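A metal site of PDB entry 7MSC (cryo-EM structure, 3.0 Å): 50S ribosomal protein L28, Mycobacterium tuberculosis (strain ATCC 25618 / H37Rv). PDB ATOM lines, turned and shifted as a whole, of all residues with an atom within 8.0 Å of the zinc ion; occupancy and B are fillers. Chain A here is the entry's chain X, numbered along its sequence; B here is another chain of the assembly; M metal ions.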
ATOM      1  N   VAL A   4      -9.241 -15.715  13.315  1.00  0.00           N
ATOM      2  CA  VAL A   4     -10.277 -16.733  13.215  1.00  0.00           C
ATOM      3  C   VAL A   4     -10.519 -17.284  14.611  1.00  0.00           C
ATOM      4  O   VAL A   4      -9.561 -17.667  15.292  1.00  0.00           O
ATOM      5  CB  VAL A   4      -9.878 -17.886  12.271  1.00  0.00           C
ATOM      6  CG1 VAL A   4     -10.901 -18.982  12.296  1.00  0.00           C
ATOM      7  CG2 VAL A   4      -9.713 -17.399  10.867  1.00  0.00           C
ATOM      8  N   CYS A   5     -11.767 -17.315  15.038  1.00  0.00           N
ATOM      9  CA  CYS A   5     -12.088 -17.876  16.341  1.00  0.00           C
ATOM     10  C   CYS A   5     -11.924 -19.389  16.321  1.00  0.00           C
ATOM     11  O   CYS A   5     -12.120 -20.047  15.305  1.00  0.00           O
ATOM     12  CB  CYS A   5     -13.508 -17.518  16.744  1.00  0.00           C
ATOM     13  SG  CYS A   5     -13.977 -18.078  18.391  1.00  0.00           S
ATOM     14  N   ASP A   6     -11.541 -19.940  17.473  1.00  0.00           N
ATOM     15  CA  ASP A   6     -11.336 -21.377  17.615  1.00  0.00           C
ATOM     16  C   ASP A   6     -12.519 -22.079  18.270  1.00  0.00           C
ATOM     17  O   ASP A   6     -12.365 -23.177  18.787  1.00  0.00           O
ATOM     18  CB  ASP A   6     -10.071 -21.665  18.426  1.00  0.00           C
ATOM     19  CG  ASP A   6      -8.807 -21.421  17.638  1.00  0.00           C
ATOM     20  OD1 ASP A   6      -8.860 -21.527  16.400  1.00  0.00           O
ATOM     21  OD2 ASP A   6      -7.766 -21.119  18.249  1.00  0.00           O
ATOM     22  N   ILE A   7     -13.685 -21.447  18.275  1.00  0.00           N
ATOM     23  CA  ILE A   7     -14.898 -22.097  18.754  1.00  0.00           C
ATOM     24  C   ILE A   7     -15.955 -22.046  17.671  1.00  0.00           C
ATOM     25  O   ILE A   7     -16.451 -23.096  17.232  1.00  0.00           O
ATOM     26  CB  ILE A   7     -15.424 -21.440  20.032  1.00  0.00           C
ATOM     27  CG1 ILE A   7     -14.405 -21.565  21.154  1.00  0.00           C
ATOM     28  CG2 ILE A   7     -16.712 -22.088  20.458  1.00  0.00           C
ATOM     29  CD1 ILE A   7     -14.786 -20.772  22.328  1.00  0.00           C
ATOM     30  N   CYS A   8     -16.308 -20.850  17.246  1.00  0.00           N
ATOM     31  CA  CYS A   8     -17.406 -20.659  16.306  1.00  0.00           C
ATOM     32  C   CYS A   8     -16.948 -20.430  14.882  1.00  0.00           C
ATOM     33  O   CYS A   8     -17.792 -20.316  13.986  1.00  0.00           O
ATOM     34  CB  CYS A   8     -18.280 -19.490  16.758  1.00  0.00           C
ATOM     35  SG  CYS A   8     -17.429 -17.917  16.795  1.00  0.00           S
ATOM     36  N   GLY A   9     -15.651 -20.358  14.624  1.00  0.00           N
ATOM     37  CA  GLY A   9     -15.186 -20.218  13.266  1.00  0.00           C
ATOM     38  C   GLY A   9     -15.408 -18.861  12.658  1.00  0.00           C
ATOM     39  O   GLY A   9     -15.378 -18.740  11.436  1.00  0.00           O
ATOM     40  N   LYS A  10     -15.632 -17.840  13.469  1.00  0.00           N
ATOM     41  CA  LYS A  10     -15.916 -16.504  12.966  1.00  0.00           C
ATOM     42  C   LYS A  10     -14.647 -15.897  12.389  1.00  0.00           C
ATOM     43  O   LYS A  10     -13.717 -15.583  13.122  1.00  0.00           O
ATOM     44  CB  LYS A  10     -16.474 -15.639  14.078  1.00  0.00           C
ATOM     45  CG  LYS A  10     -16.795 -14.251  13.642  1.00  0.00           C
ATOM     46  CD  LYS A  10     -17.710 -13.531  14.626  1.00  0.00           C
ATOM     47  CE  LYS A  10     -16.993 -12.997  15.811  1.00  0.00           C
ATOM     48  NZ  LYS A  10     -17.951 -12.158  16.564  1.00  0.00           N
ATOM     49  N   GLY A  11     -14.612 -15.715  11.080  1.00  0.00           N
ATOM     50  CA  GLY A  11     -13.470 -15.155  10.421  1.00  0.00           C
ATOM     51  C   GLY A  11     -13.702 -13.742   9.948  1.00  0.00           C
ATOM     52  O   GLY A  11     -14.683 -13.100  10.300  1.00  0.00           O
ATOM     53  N   PRO A  31     -11.967 -10.059  13.105  1.00  0.00           N
ATOM     54  CA  PRO A  31     -12.666 -10.140  14.387  1.00  0.00           C
ATOM     55  C   PRO A  31     -11.721  -9.871  15.547  1.00  0.00           C
ATOM     56  O   PRO A  31     -10.503  -9.929  15.420  1.00  0.00           O
ATOM     57  CB  PRO A  31     -13.174 -11.571  14.409  1.00  0.00           C
ATOM     58  CG  PRO A  31     -12.293 -12.297  13.529  1.00  0.00           C
ATOM     59  CD  PRO A  31     -11.895 -11.373  12.451  1.00  0.00           C
ATOM     60  N   ASN A  32     -12.323  -9.590  16.701  1.00  0.00           N
ATOM     61  CA  ASN A  32     -11.556  -9.203  17.873  1.00  0.00           C
ATOM     62  C   ASN A  32     -11.114 -10.479  18.577  1.00  0.00           C
ATOM     63  O   ASN A  32     -11.690 -10.925  19.566  1.00  0.00           O
ATOM     64  CB  ASN A  32     -12.385  -8.331  18.798  1.00  0.00           C
ATOM     65  CG  ASN A  32     -11.554  -7.661  19.861  1.00  0.00           C
ATOM     66  OD1 ASN A  32     -10.347  -7.828  19.919  1.00  0.00           O
ATOM     67  ND2 ASN A  32     -12.211  -6.902  20.704  1.00  0.00           N
ATOM     68  N   ILE A  33     -10.042 -11.060  18.051  1.00  0.00           N
ATOM     69  CA  ILE A  33      -9.549 -12.336  18.529  1.00  0.00           C
ATOM     70  C   ILE A  33      -8.576 -12.080  19.667  1.00  0.00           C
ATOM     71  O   ILE A  33      -7.503 -11.510  19.456  1.00  0.00           O
ATOM     72  CB  ILE A  33      -8.908 -13.128  17.404  1.00  0.00           C
ATOM     73  CG1 ILE A  33      -9.944 -13.475  16.337  1.00  0.00           C
ATOM     74  CG2 ILE A  33      -8.282 -14.364  17.943  1.00  0.00           C
ATOM     75  CD1 ILE A  33     -11.059 -14.316  16.837  1.00  0.00           C
ATOM     76  N   ASN A  50      -7.516 -19.105  20.825  1.00  0.00           N
ATOM     77  CA  ASN A  50      -7.809 -17.832  20.199  1.00  0.00           C
ATOM     78  C   ASN A  50      -9.325 -17.729  20.083  1.00  0.00           C
ATOM     79  O   ASN A  50      -9.918 -18.320  19.176  1.00  0.00           O
ATOM     80  CB  ASN A  50      -7.175 -17.732  18.824  1.00  0.00           C
ATOM     81  CG  ASN A  50      -5.711 -17.563  18.879  1.00  0.00           C
ATOM     82  OD1 ASN A  50      -5.179 -16.886  19.756  1.00  0.00           O
ATOM     83  ND2 ASN A  50      -5.016 -18.152  17.921  1.00  0.00           N
ATOM     84  N   VAL A  51      -9.949 -17.001  20.982  1.00  0.00           N
ATOM     85  CA  VAL A  51     -11.394 -16.853  20.963  1.00  0.00           C
ATOM     86  C   VAL A  51     -11.742 -15.407  20.643  1.00  0.00           C
ATOM     87  O   VAL A  51     -10.957 -14.491  20.859  1.00  0.00           O
ATOM     88  CB  VAL A  51     -12.034 -17.284  22.291  1.00  0.00           C
ATOM     89  CG1 VAL A  51     -11.704 -18.713  22.573  1.00  0.00           C
ATOM     90  CG2 VAL A  51     -11.529 -16.434  23.381  1.00  0.00           C
ATOM     91  N   CYS A  52     -12.928 -15.218  20.082  1.00  0.00           N
ATOM     92  CA  CYS A  52     -13.374 -13.870  19.835  1.00  0.00           C
ATOM     93  C   CYS A  52     -14.021 -13.319  21.097  1.00  0.00           C
ATOM     94  O   CYS A  52     -14.269 -14.044  22.063  1.00  0.00           O
ATOM     95  CB  CYS A  52     -14.347 -13.820  18.664  1.00  0.00           C
ATOM     96  SG  CYS A  52     -15.894 -14.652  18.930  1.00  0.00           S
ATOM     97  N   THR A  53     -14.290 -12.026  21.093  1.00  0.00           N
ATOM     98  CA  THR A  53     -14.822 -11.421  22.299  1.00  0.00           C
ATOM     99  C   THR A  53     -16.310 -11.631  22.465  1.00  0.00           C
ATOM    100  O   THR A  53     -16.832 -11.374  23.549  1.00  0.00           O
ATOM    101  CB  THR A  53     -14.518  -9.931  22.318  1.00  0.00           C
ATOM    102  OG1 THR A  53     -15.047  -9.337  21.130  1.00  0.00           O
ATOM    103  CG2 THR A  53     -13.047  -9.714  22.385  1.00  0.00           C
ATOM    104  N   SER A  54     -17.000 -12.089  21.432  1.00  0.00           N
ATOM    105  CA  SER A  54     -18.393 -12.447  21.601  1.00  0.00           C
ATOM    106  C   SER A  54     -18.561 -13.785  22.304  1.00  0.00           C
ATOM    107  O   SER A  54     -19.650 -14.080  22.792  1.00  0.00           O
ATOM    108  CB  SER A  54     -19.089 -12.475  20.242  1.00  0.00           C
ATOM    109  OG  SER A  54     -18.559 -13.514  19.444  1.00  0.00           O
ATOM    110  N   CYS A  55     -17.499 -14.592  22.368  1.00  0.00           N
ATOM    111  CA  CYS A  55     -17.517 -15.852  23.092  1.00  0.00           C
ATOM    112  C   CYS A  55     -16.987 -15.744  24.511  1.00  0.00           C
ATOM    113  O   CYS A  55     -17.329 -16.576  25.347  1.00  0.00           O
ATOM    114  CB  CYS A  55     -16.721 -16.912  22.331  1.00  0.00           C
ATOM    115  SG  CYS A  55     -17.437 -17.345  20.749  1.00  0.00           S
ATOM    116  N   ILE A  56     -16.155 -14.746  24.798  1.00  0.00           N
ATOM    117  CA  ILE A  56     -15.823 -14.461  26.183  1.00  0.00           C
ATOM    118  C   ILE A  56     -17.015 -13.828  26.884  1.00  0.00           C
ATOM    119  O   ILE A  56     -17.216 -14.020  28.086  1.00  0.00           O
ATOM    120  CB  ILE A  56     -14.590 -13.537  26.240  1.00  0.00           C
ATOM    121  CG1 ILE A  56     -13.462 -14.153  25.456  1.00  0.00           C
ATOM    122  CG2 ILE A  56     -14.098 -13.379  27.645  1.00  0.00           C
ATOM    123  CD1 ILE A  56     -12.340 -13.199  25.223  1.00  0.00           C
ATOM    124  N   LYS A  60     -18.805 -19.400  26.760  1.00  0.00           N
ATOM    125  CA  LYS A  60     -18.258 -20.443  25.901  1.00  0.00           C
ATOM    126  C   LYS A  60     -16.959 -21.006  26.461  1.00  0.00           C
ATOM    127  O   LYS A  60     -16.598 -22.146  26.154  1.00  0.00           O
ATOM    128  CB  LYS A  60     -18.001 -19.892  24.503  1.00  0.00           C
ATOM    129  CG  LYS A  60     -19.173 -19.274  23.773  1.00  0.00           C
ATOM    130  CD  LYS A  60     -20.125 -20.276  23.155  1.00  0.00           C
ATOM    131  CE  LYS A  60     -21.395 -20.415  23.969  1.00  0.00           C
ATOM    132  NZ  LYS A  60     -22.393 -21.249  23.263  1.00  0.00           N
ATOM    133  P     U B 486     -16.350  -9.145  15.834  1.00  0.00           P
ATOM    134  OP1   U B 486     -15.301  -9.837  16.610  1.00  0.00           O
ATOM    135  OP2   U B 486     -17.739  -9.605  15.937  1.00  0.00           O
ATOM    136  O5'   U B 486     -16.345  -7.618  16.252  1.00  0.00           O
ATOM    137  C5'   U B 486     -15.146  -6.934  16.540  1.00  0.00           C
ATOM    138  C4'   U B 486     -15.399  -5.507  16.924  1.00  0.00           C
ATOM    139  O4'   U B 486     -16.096  -4.830  15.856  1.00  0.00           O
ATOM    140  C3'   U B 486     -16.294  -5.275  18.130  1.00  0.00           C
ATOM    141  O3'   U B 486     -15.635  -5.451  19.350  1.00  0.00           O
ATOM    142  C2'   U B 486     -16.769  -3.857  17.899  1.00  0.00           C
ATOM    143  O2'   U B 486     -15.740  -2.937  18.235  1.00  0.00           O
ATOM    144  C1'   U B 486     -16.947  -3.836  16.388  1.00  0.00           C
ATOM    145  N1    U B 486     -18.344  -4.119  16.009  1.00  0.00           N
ATOM    146  C2    U B 486     -19.227  -3.078  16.083  1.00  0.00           C
ATOM    147  O2    U B 486     -18.925  -1.954  16.433  1.00  0.00           O
ATOM    148  N3    U B 486     -20.502  -3.382  15.722  1.00  0.00           N
ATOM    149  C4    U B 486     -20.985  -4.597  15.323  1.00  0.00           C
ATOM    150  O4    U B 486     -22.172  -4.707  15.036  1.00  0.00           O
ATOM    151  C5    U B 486     -20.023  -5.618  15.273  1.00  0.00           C
ATOM    152  C6    U B 486     -18.765  -5.339  15.593  1.00  0.00           C
HETATM  153 ZN    ZN M   1     -16.174 -17.079  18.696  1.00  0.00          ZN
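The zinc ion is bound by the side-chain sulfur of Cys 55, the side-chain sulfur of Cys 8, the side-chain sulfur of Cys 5 and the side-chain sulfur of Cys 52.
The zinc ion has four donor atoms within binding distance.
Of the 20 residues printed, 4 come within 4 Å of the zinc ion.
The nearest printed residue that does not touch the zinc ion is Ser 54 (4.4 Å).
The backbone NH (N) of Lys 60 lies within hydrogen-bond range of the backbone carbonyl oxygen (O) of Cys 55, 3.5 Å away.
SG of Cys 52 sits close to OG of Ser 54 (2.9 Å).
N of Cys 5 is in hydrogen-bond range of O of Lys 10 (3.2 Å).
SG of Cys 5 lies close to N of Ile 7 (3.4 Å).
SG of Cys 8 lies close to N of Lys 10, at 3.8 Å.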
